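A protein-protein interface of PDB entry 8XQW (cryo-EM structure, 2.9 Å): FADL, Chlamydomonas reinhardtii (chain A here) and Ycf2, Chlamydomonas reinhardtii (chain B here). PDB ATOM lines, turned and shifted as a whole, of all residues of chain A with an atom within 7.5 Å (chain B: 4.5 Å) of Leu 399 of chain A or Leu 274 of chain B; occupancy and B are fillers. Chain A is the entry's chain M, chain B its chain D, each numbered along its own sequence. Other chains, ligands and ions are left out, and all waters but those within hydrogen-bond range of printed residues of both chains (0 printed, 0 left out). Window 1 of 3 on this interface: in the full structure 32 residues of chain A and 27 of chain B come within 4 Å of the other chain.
Hydrophobic or aromatic side chains of chain B that line the printed part of chain A: Leu 270, Leu 274 and Leu 278. Along chain B the printed residues that touch a printed residue of chain A span positions 270 to 278. Hydrophobic or aromatic side chains of chain A that line the printed part of chain B: Met 366, Leu 396, Leu 399 and His 400. Among the printed residues, 4 pairs touch across the chains. Among the printed residues, no Asp or Glu carboxylate lies within 4 Å of a Lys or Arg side-chain nitrogen of the other chain.
Ser 393 of chain A touches none of the printed residues of chain B. Of the printed residues of chain B, Leu 396 of chain A touches Gln 271. His 397 of chain A touches none of the printed residues of chain B. Of chain B, only Leu 274 comes within 4 Å of Leu 399 of chain A. Of the printed residues of chain B, His 400 of chain A touches Leu 270. Of the printed residues of chain A, Leu 270 of chain B touches His 400 (3.8 Å). Printed residues of chain A within 4 Å of Gln 271 of chain B: Leu 396 (3.8 Å). Leu 274 of chain B touches just one residue of chain A: Leu 399 (3.8 Å). Printed residues of chain A within 4 Å of Leu 278 of chain B: Met 366. The nearest residue of chain A that does not touch Leu 274 of chain B is Arg 395 of chain A (4.5 Å). The nearest printed residue of chain B that does not touch Met 366 of chain A is Leu 274 of chain B (5.8 Å).
Among the printed residues, pairs that only touch across the chains: Met 366 of chain A with Leu 278 of chain B (3.6 Å), Leu 396 of chain A with Gln 271 of chain B (3.8 Å), Leu 399 of chain A with Leu 274 of chain B (3.8 Å) and His 400 of chain A with Leu 270 of chain B (3.8 Å).
O of His 400 of chain A lies within hydrogen-bond range of ND1 of His 404 of chain A.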
ATOM      1  N   ALA A 364     -36.081  16.263  21.622  1.00  0.00           N
ATOM      2  CA  ALA A 364     -34.860  17.027  21.390  1.00  0.00           C
ATOM      3  C   ALA A 364     -34.219  16.678  20.056  1.00  0.00           C
ATOM      4  O   ALA A 364     -33.656  17.552  19.395  1.00  0.00           O
ATOM      5  CB  ALA A 364     -33.866  16.807  22.521  1.00  0.00           C
ATOM      6  N   MET A 365     -34.282  15.415  19.648  1.00  0.00           N
ATOM      7  CA  MET A 365     -33.768  15.001  18.350  1.00  0.00           C
ATOM      8  C   MET A 365     -34.789  15.144  17.235  1.00  0.00           C
ATOM      9  O   MET A 365     -34.564  14.606  16.150  1.00  0.00           O
ATOM     10  CB  MET A 365     -33.289  13.558  18.406  1.00  0.00           C
ATOM     11  CG  MET A 365     -32.423  13.256  19.588  1.00  0.00           C
ATOM     12  SD  MET A 365     -30.939  14.257  19.599  1.00  0.00           S
ATOM     13  CE  MET A 365     -30.025  13.479  18.285  1.00  0.00           C
ATOM     14  N   MET A 366     -35.907  15.816  17.483  1.00  0.00           N
ATOM     15  CA  MET A 366     -36.846  16.227  16.440  1.00  0.00           C
ATOM     16  C   MET A 366     -37.522  15.040  15.762  1.00  0.00           C
ATOM     17  O   MET A 366     -37.819  15.089  14.573  1.00  0.00           O
ATOM     18  CB  MET A 366     -36.157  17.111  15.402  1.00  0.00           C
ATOM     19  CG  MET A 366     -35.874  18.509  15.886  1.00  0.00           C
ATOM     20  SD  MET A 366     -34.482  19.260  15.035  1.00  0.00           S
ATOM     21  CE  MET A 366     -33.196  18.067  15.369  1.00  0.00           C
ATOM     22  N   PRO A 392     -31.575  22.643  24.372  1.00  0.00           N
ATOM     23  CA  PRO A 392     -30.576  22.842  23.316  1.00  0.00           C
ATOM     24  C   PRO A 392     -29.217  22.277  23.659  1.00  0.00           C
ATOM     25  O   PRO A 392     -28.574  21.648  22.809  1.00  0.00           O
ATOM     26  CB  PRO A 392     -30.534  24.363  23.177  1.00  0.00           C
ATOM     27  CG  PRO A 392     -31.801  24.824  23.716  1.00  0.00           C
ATOM     28  CD  PRO A 392     -32.092  23.933  24.844  1.00  0.00           C
ATOM     29  N   SER A 393     -28.753  22.484  24.884  1.00  0.00           N
ATOM     30  CA  SER A 393     -27.475  21.915  25.273  1.00  0.00           C
ATOM     31  C   SER A 393     -27.514  20.399  25.237  1.00  0.00           C
ATOM     32  O   SER A 393     -26.518  19.757  24.899  1.00  0.00           O
ATOM     33  CB  SER A 393     -27.098  22.406  26.657  1.00  0.00           C
ATOM     34  OG  SER A 393     -27.540  23.732  26.838  1.00  0.00           O
ATOM     35  N   TRP A 394     -28.653  19.804  25.580  1.00  0.00           N
ATOM     36  CA  TRP A 394     -28.756  18.353  25.521  1.00  0.00           C
ATOM     37  C   TRP A 394     -28.634  17.865  24.093  1.00  0.00           C
ATOM     38  O   TRP A 394     -27.927  16.892  23.815  1.00  0.00           O
ATOM     39  CB  TRP A 394     -30.074  17.891  26.124  1.00  0.00           C
ATOM     40  CG  TRP A 394     -30.286  16.438  25.998  1.00  0.00           C
ATOM     41  CD1 TRP A 394     -30.865  15.789  24.965  1.00  0.00           C
ATOM     42  CD2 TRP A 394     -29.918  15.440  26.945  1.00  0.00           C
ATOM     43  NE1 TRP A 394     -30.882  14.446  25.202  1.00  0.00           N
ATOM     44  CE2 TRP A 394     -30.300  14.209  26.415  1.00  0.00           C
ATOM     45  CE3 TRP A 394     -29.296  15.470  28.189  1.00  0.00           C
ATOM     46  CZ2 TRP A 394     -30.087  13.023  27.080  1.00  0.00           C
ATOM     47  CZ3 TRP A 394     -29.086  14.296  28.845  1.00  0.00           C
ATOM     48  CH2 TRP A 394     -29.480  13.089  28.296  1.00  0.00           C
ATOM     49  N   ARG A 395     -29.337  18.518  23.173  1.00  0.00           N
ATOM     50  CA  ARG A 395     -29.211  18.169  21.765  1.00  0.00           C
ATOM     51  C   ARG A 395     -27.762  18.232  21.317  1.00  0.00           C
ATOM     52  O   ARG A 395     -27.271  17.328  20.632  1.00  0.00           O
ATOM     53  CB  ARG A 395     -30.070  19.105  20.928  1.00  0.00           C
ATOM     54  CG  ARG A 395     -29.920  18.909  19.464  1.00  0.00           C
ATOM     55  CD  ARG A 395     -30.610  20.002  18.710  1.00  0.00           C
ATOM     56  NE  ARG A 395     -32.009  20.120  19.084  1.00  0.00           N
ATOM     57  CZ  ARG A 395     -32.587  21.264  19.425  1.00  0.00           C
ATOM     58  NH1 ARG A 395     -31.883  22.382  19.439  1.00  0.00           N
ATOM     59  NH2 ARG A 395     -33.868  21.295  19.746  1.00  0.00           N
ATOM     60  N   LEU A 396     -27.055  19.285  21.713  1.00  0.00           N
ATOM     61  CA  LEU A 396     -25.673  19.450  21.273  1.00  0.00           C
ATOM     62  C   LEU A 396     -24.779  18.354  21.817  1.00  0.00           C
ATOM     63  O   LEU A 396     -23.974  17.772  21.085  1.00  0.00           O
ATOM     64  CB  LEU A 396     -25.147  20.806  21.705  1.00  0.00           C
ATOM     65  CG  LEU A 396     -25.523  21.962  20.811  1.00  0.00           C
ATOM     66  CD1 LEU A 396     -24.840  23.182  21.320  1.00  0.00           C
ATOM     67  CD2 LEU A 396     -25.093  21.659  19.413  1.00  0.00           C
ATOM     68  N   HIS A 397     -24.881  18.074  23.109  1.00  0.00           N
ATOM     69  CA  HIS A 397     -24.010  17.066  23.692  1.00  0.00           C
ATOM     70  C   HIS A 397     -24.313  15.685  23.143  1.00  0.00           C
ATOM     71  O   HIS A 397     -23.398  14.888  22.927  1.00  0.00           O
ATOM     72  CB  HIS A 397     -24.141  17.085  25.205  1.00  0.00           C
ATOM     73  CG  HIS A 397     -23.906  18.432  25.809  1.00  0.00           C
ATOM     74  ND1 HIS A 397     -24.614  18.893  26.891  1.00  0.00           N
ATOM     75  CD2 HIS A 397     -23.043  19.418  25.478  1.00  0.00           C
ATOM     76  CE1 HIS A 397     -24.203  20.108  27.199  1.00  0.00           C
ATOM     77  NE2 HIS A 397     -23.248  20.449  26.357  1.00  0.00           N
ATOM     78  N   HIS A 398     -25.577  15.390  22.865  1.00  0.00           N
ATOM     79  CA  HIS A 398     -25.890  14.080  22.315  1.00  0.00           C
ATOM     80  C   HIS A 398     -25.386  13.937  20.885  1.00  0.00           C
ATOM     81  O   HIS A 398     -24.878  12.877  20.512  1.00  0.00           O
ATOM     82  CB  HIS A 398     -27.384  13.819  22.376  1.00  0.00           C
ATOM     83  CG  HIS A 398     -27.744  12.413  22.041  1.00  0.00           C
ATOM     84  ND1 HIS A 398     -27.065  11.335  22.556  1.00  0.00           N
ATOM     85  CD2 HIS A 398     -28.685  11.907  21.215  1.00  0.00           C
ATOM     86  CE1 HIS A 398     -27.579  10.222  22.073  1.00  0.00           C
ATOM     87  NE2 HIS A 398     -28.563  10.541  21.254  1.00  0.00           N
ATOM     88  N   LEU A 399     -25.535  14.972  20.059  1.00  0.00           N
ATOM     89  CA  LEU A 399     -24.970  14.904  18.717  1.00  0.00           C
ATOM     90  C   LEU A 399     -23.465  14.711  18.768  1.00  0.00           C
ATOM     91  O   LEU A 399     -22.907  13.880  18.039  1.00  0.00           O
ATOM     92  CB  LEU A 399     -25.315  16.160  17.936  1.00  0.00           C
ATOM     93  CG  LEU A 399     -26.756  16.275  17.466  1.00  0.00           C
ATOM     94  CD1 LEU A 399     -27.014  17.630  16.873  1.00  0.00           C
ATOM     95  CD2 LEU A 399     -27.042  15.211  16.458  1.00  0.00           C
ATOM     96  N   HIS A 400     -22.784  15.465  19.627  1.00  0.00           N
ATOM     97  CA  HIS A 400     -21.344  15.303  19.761  1.00  0.00           C
ATOM     98  C   HIS A 400     -20.991  13.899  20.214  1.00  0.00           C
ATOM     99  O   HIS A 400     -19.932  13.377  19.865  1.00  0.00           O
ATOM    100  CB  HIS A 400     -20.797  16.335  20.739  1.00  0.00           C
ATOM    101  CG  HIS A 400     -19.347  16.171  21.054  1.00  0.00           C
ATOM    102  ND1 HIS A 400     -18.386  17.033  20.583  1.00  0.00           N
ATOM    103  CD2 HIS A 400     -18.694  15.256  21.807  1.00  0.00           C
ATOM    104  CE1 HIS A 400     -17.202  16.652  21.025  1.00  0.00           C
ATOM    105  NE2 HIS A 400     -17.360  15.576  21.768  1.00  0.00           N
ATOM    106  N   HIS A 401     -21.860  13.272  20.998  1.00  0.00           N
ATOM    107  CA  HIS A 401     -21.600  11.899  21.419  1.00  0.00           C
ATOM    108  C   HIS A 401     -21.754  10.928  20.259  1.00  0.00           C
ATOM    109  O   HIS A 401     -20.911  10.050  20.061  1.00  0.00           O
ATOM    110  CB  HIS A 401     -22.541  11.532  22.561  1.00  0.00           C
ATOM    111  CG  HIS A 401     -22.579  10.074  22.874  1.00  0.00           C
ATOM    112  ND1 HIS A 401     -21.448   9.340  23.137  1.00  0.00           N
ATOM    113  CD2 HIS A 401     -23.619   9.217  22.987  1.00  0.00           C
ATOM    114  CE1 HIS A 401     -21.786   8.090  23.387  1.00  0.00           C
ATOM    115  NE2 HIS A 401     -23.098   7.989  23.302  1.00  0.00           N
ATOM    116  N   LEU A 402     -22.820  11.070  19.481  1.00  0.00           N
ATOM    117  CA  LEU A 402     -23.010  10.208  18.324  1.00  0.00           C
ATOM    118  C   LEU A 402     -21.883  10.326  17.317  1.00  0.00           C
ATOM    119  O   LEU A 402     -21.595   9.356  16.615  1.00  0.00           O
ATOM    120  CB  LEU A 402     -24.317  10.533  17.618  1.00  0.00           C
ATOM    121  CG  LEU A 402     -25.609  10.224  18.338  1.00  0.00           C
ATOM    122  CD1 LEU A 402     -26.751  10.700  17.495  1.00  0.00           C
ATOM    123  CD2 LEU A 402     -25.696   8.754  18.574  1.00  0.00           C
ATOM    124  N   LEU A 403     -21.261  11.494  17.203  1.00  0.00           N
ATOM    125  CA  LEU A 403     -20.198  11.652  16.222  1.00  0.00           C
ATOM    126  C   LEU A 403     -18.873  11.063  16.674  1.00  0.00           C
ATOM    127  O   LEU A 403     -17.999  10.837  15.835  1.00  0.00           O
ATOM    128  CB  LEU A 403     -20.000  13.127  15.898  1.00  0.00           C
ATOM    129  CG  LEU A 403     -21.123  13.811  15.131  1.00  0.00           C
ATOM    130  CD1 LEU A 403     -20.996  15.296  15.260  1.00  0.00           C
ATOM    131  CD2 LEU A 403     -21.059  13.422  13.690  1.00  0.00           C
ATOM    132  N   HIS A 404     -18.697  10.810  17.966  1.00  0.00           N
ATOM    133  CA  HIS A 404     -17.410  10.419  18.520  1.00  0.00           C
ATOM    134  C   HIS A 404     -17.506   9.163  19.370  1.00  0.00           C
ATOM    135  O   HIS A 404     -16.736   8.997  20.311  1.00  0.00           O
ATOM    136  CB  HIS A 404     -16.829  11.544  19.364  1.00  0.00           C
ATOM    137  CG  HIS A 404     -16.428  12.746  18.580  1.00  0.00           C
ATOM    138  ND1 HIS A 404     -17.306  13.758  18.270  1.00  0.00           N
ATOM    139  CD2 HIS A 404     -15.239  13.106  18.053  1.00  0.00           C
ATOM    140  CE1 HIS A 404     -16.676  14.689  17.580  1.00  0.00           C
ATOM    141  NE2 HIS A 404     -15.419  14.318  17.435  1.00  0.00           N
ATOM    142  N   THR A 405     -18.435   8.275  19.059  1.00  0.00           N
ATOM    143  CA  THR A 405     -18.714   7.157  19.947  1.00  0.00           C
ATOM    144  C   THR A 405     -17.483   6.285  20.123  1.00  0.00           C
ATOM    145  O   THR A 405     -16.889   5.837  19.142  1.00  0.00           O
ATOM    146  CB  THR A 405     -19.873   6.340  19.399  1.00  0.00           C
ATOM    147  OG1 THR A 405     -21.005   7.192  19.229  1.00  0.00           O
ATOM    148  CG2 THR A 405     -20.240   5.260  20.360  1.00  0.00           C
ATOM    149  N   TRP A 413     -18.722  13.225  26.508  1.00  0.00           N
ATOM    150  CA  TRP A 413     -20.109  13.215  26.936  1.00  0.00           C
ATOM    151  C   TRP A 413     -20.642  11.810  27.107  1.00  0.00           C
ATOM    152  O   TRP A 413     -21.849  11.594  27.007  1.00  0.00           O
ATOM    153  CB  TRP A 413     -20.961  14.006  25.954  1.00  0.00           C
ATOM    154  CG  TRP A 413     -20.609  15.418  26.013  1.00  0.00           C
ATOM    155  CD1 TRP A 413     -20.014  16.147  25.050  1.00  0.00           C
ATOM    156  CD2 TRP A 413     -20.772  16.280  27.131  1.00  0.00           C
ATOM    157  NE1 TRP A 413     -19.810  17.423  25.485  1.00  0.00           N
ATOM    158  CE2 TRP A 413     -20.270  17.528  26.768  1.00  0.00           C
ATOM    159  CE3 TRP A 413     -21.309  16.119  28.406  1.00  0.00           C
ATOM    160  CZ2 TRP A 413     -20.290  18.607  27.625  1.00  0.00           C
ATOM    161  CZ3 TRP A 413     -21.324  17.181  29.247  1.00  0.00           C
ATOM    162  CH2 TRP A 413     -20.820  18.412  28.860  1.00  0.00           C
ATOM    163  N   PRO A 578     -31.406   7.513  12.541  1.00  0.00           N
ATOM    164  CA  PRO A 578     -31.667   8.518  13.580  1.00  0.00           C
ATOM    165  C   PRO A 578     -33.054   9.115  13.541  1.00  0.00           C
ATOM    166  O   PRO A 578     -33.435   9.786  14.503  1.00  0.00           O
ATOM    167  CB  PRO A 578     -30.601   9.582  13.306  1.00  0.00           C
ATOM    168  CG  PRO A 578     -29.542   8.871  12.573  1.00  0.00           C
ATOM    169  CD  PRO A 578     -30.249   7.878  11.716  1.00  0.00           C
ATOM    170  N   PHE B  48     -25.807  14.666   7.580  1.00  0.00           N
ATOM    171  CA  PHE B  48     -24.980  15.448   8.495  1.00  0.00           C
ATOM    172  C   PHE B  48     -23.966  14.567   9.209  1.00  0.00           C
ATOM    173  O   PHE B  48     -22.768  14.876   9.254  1.00  0.00           O
ATOM    174  CB  PHE B  48     -25.872  16.170   9.499  1.00  0.00           C
ATOM    175  CG  PHE B  48     -25.167  16.588  10.744  1.00  0.00           C
ATOM    176  CD1 PHE B  48     -24.171  17.539  10.705  1.00  0.00           C
ATOM    177  CD2 PHE B  48     -25.513  16.049  11.957  1.00  0.00           C
ATOM    178  CE1 PHE B  48     -23.526  17.931  11.853  1.00  0.00           C
ATOM    179  CE2 PHE B  48     -24.873  16.438  13.105  1.00  0.00           C
ATOM    180  CZ  PHE B  48     -23.878  17.379  13.052  1.00  0.00           C
ATOM    181  N   LEU B 270     -19.709  22.532  15.099  1.00  0.00           N
ATOM    182  CA  LEU B 270     -20.844  21.622  15.160  1.00  0.00           C
ATOM    183  C   LEU B 270     -22.150  22.356  14.902  1.00  0.00           C
ATOM    184  O   LEU B 270     -22.987  21.899  14.121  1.00  0.00           O
ATOM    185  CB  LEU B 270     -20.879  20.938  16.519  1.00  0.00           C
ATOM    186  CG  LEU B 270     -21.468  19.543  16.648  1.00  0.00           C
ATOM    187  CD1 LEU B 270     -21.017  18.972  17.946  1.00  0.00           C
ATOM    188  CD2 LEU B 270     -22.955  19.604  16.630  1.00  0.00           C
ATOM    189  N   GLN B 271     -22.341  23.498  15.552  1.00  0.00           N
ATOM    190  CA  GLN B 271     -23.584  24.234  15.383  1.00  0.00           C
ATOM    191  C   GLN B 271     -23.710  24.784  13.976  1.00  0.00           C
ATOM    192  O   GLN B 271     -24.806  24.808  13.410  1.00  0.00           O
ATOM    193  CB  GLN B 271     -23.662  25.365  16.390  1.00  0.00           C
ATOM    194  CG  GLN B 271     -23.840  24.909  17.790  1.00  0.00           C
ATOM    195  CD  GLN B 271     -24.220  26.028  18.692  1.00  0.00           C
ATOM    196  OE1 GLN B 271     -25.389  26.325  18.873  1.00  0.00           O
ATOM    197  NE2 GLN B 271     -23.230  26.663  19.266  1.00  0.00           N
ATOM    198  N   LYS B 272     -22.599  25.222  13.393  1.00  0.00           N
ATOM    199  CA  LYS B 272     -22.638  25.731  12.027  1.00  0.00           C
ATOM    200  C   LYS B 272     -23.041  24.639  11.043  1.00  0.00           C
ATOM    201  O   LYS B 272     -23.958  24.823  10.231  1.00  0.00           O
ATOM    202  CB  LYS B 272     -21.280  26.326  11.683  1.00  0.00           C
ATOM    203  CG  LYS B 272     -20.943  26.357  10.236  1.00  0.00           C
ATOM    204  CD  LYS B 272     -19.616  27.039  10.055  1.00  0.00           C
ATOM    205  CE  LYS B 272     -18.908  26.525   8.831  1.00  0.00           C
ATOM    206  NZ  LYS B 272     -17.646  27.272   8.595  1.00  0.00           N
ATOM    207  N   LEU B 273     -22.375  23.486  11.112  1.00  0.00           N
ATOM    208  CA  LEU B 273     -22.755  22.352  10.276  1.00  0.00           C
ATOM    209  C   LEU B 273     -24.214  21.974  10.466  1.00  0.00           C
ATOM    210  O   LEU B 273     -24.932  21.727   9.492  1.00  0.00           O
ATOM    211  CB  LEU B 273     -21.868  21.158  10.597  1.00  0.00           C
ATOM    212  CG  LEU B 273     -20.868  20.718   9.544  1.00  0.00           C
ATOM    213  CD1 LEU B 273     -21.603  20.168   8.365  1.00  0.00           C
ATOM    214  CD2 LEU B 273     -20.052  21.902   9.126  1.00  0.00           C
ATOM    215  N   LEU B 274     -24.663  21.894  11.714  1.00  0.00           N
ATOM    216  CA  LEU B 274     -26.022  21.446  11.967  1.00  0.00           C
ATOM    217  C   LEU B 274     -27.036  22.401  11.371  1.00  0.00           C
ATOM    218  O   LEU B 274     -27.990  21.976  10.711  1.00  0.00           O
ATOM    219  CB  LEU B 274     -26.243  21.305  13.463  1.00  0.00           C
ATOM    220  CG  LEU B 274     -27.672  20.939  13.807  1.00  0.00           C
ATOM    221  CD1 LEU B 274     -27.979  19.589  13.222  1.00  0.00           C
ATOM    222  CD2 LEU B 274     -27.864  20.939  15.301  1.00  0.00           C
ATOM    223  N   SER B 275     -26.854  23.699  11.592  1.00  0.00           N
ATOM    224  CA  SER B 275     -27.806  24.657  11.052  1.00  0.00           C
ATOM    225  C   SER B 275     -27.782  24.659   9.535  1.00  0.00           C
ATOM    226  O   SER B 275     -28.806  24.918   8.898  1.00  0.00           O
ATOM    227  CB  SER B 275     -27.514  26.050  11.581  1.00  0.00           C
ATOM    228  OG  SER B 275     -27.990  27.018  10.669  1.00  0.00           O
ATOM    229  N   LYS B 276     -26.626  24.386   8.932  1.00  0.00           N
ATOM    230  CA  LYS B 276     -26.606  24.289   7.478  1.00  0.00           C
ATOM    231  C   LYS B 276     -27.395  23.086   6.986  1.00  0.00           C
ATOM    232  O   LYS B 276     -28.173  23.205   6.037  1.00  0.00           O
ATOM    233  CB  LYS B 276     -25.171  24.211   6.970  1.00  0.00           C
ATOM    234  CG  LYS B 276     -25.039  23.642   5.585  1.00  0.00           C
ATOM    235  CD  LYS B 276     -23.588  23.380   5.268  1.00  0.00           C
ATOM    236  CE  LYS B 276     -23.448  22.599   3.981  1.00  0.00           C
ATOM    237  NZ  LYS B 276     -22.028  22.368   3.614  1.00  0.00           N
ATOM    238  N   TYR B 277     -27.224  21.932   7.621  1.00  0.00           N
ATOM    239  CA  TYR B 277     -27.811  20.706   7.091  1.00  0.00           C
ATOM    240  C   TYR B 277     -29.265  20.505   7.463  1.00  0.00           C
ATOM    241  O   TYR B 277     -29.953  19.728   6.799  1.00  0.00           O
ATOM    242  CB  TYR B 277     -27.026  19.489   7.561  1.00  0.00           C
ATOM    243  CG  TYR B 277     -25.981  19.077   6.579  1.00  0.00           C
ATOM    244  CD1 TYR B 277     -26.314  18.353   5.457  1.00  0.00           C
ATOM    245  CD2 TYR B 277     -24.662  19.421   6.768  1.00  0.00           C
ATOM    246  CE1 TYR B 277     -25.358  17.977   4.555  1.00  0.00           C
ATOM    247  CE2 TYR B 277     -23.703  19.050   5.874  1.00  0.00           C
ATOM    248  CZ  TYR B 277     -24.054  18.329   4.770  1.00  0.00           C
ATOM    249  OH  TYR B 277     -23.081  17.959   3.876  1.00  0.00           O
ATOM    250  N   LEU B 278     -29.756  21.160   8.504  1.00  0.00           N
ATOM    251  CA  LEU B 278     -31.116  20.893   8.940  1.00  0.00           C
ATOM    252  C   LEU B 278     -32.154  21.785   8.286  1.00  0.00           C
ATOM    253  O   LEU B 278     -33.195  21.281   7.855  1.00  0.00           O
ATOM    254  CB  LEU B 278     -31.232  21.044  10.454  1.00  0.00           C
ATOM    255  CG  LEU B 278     -31.897  19.851  11.127  1.00  0.00           C
ATOM    256  CD1 LEU B 278     -31.249  18.557  10.670  1.00  0.00           C
ATOM    257  CD2 LEU B 278     -31.818  19.984  12.621  1.00  0.00           C
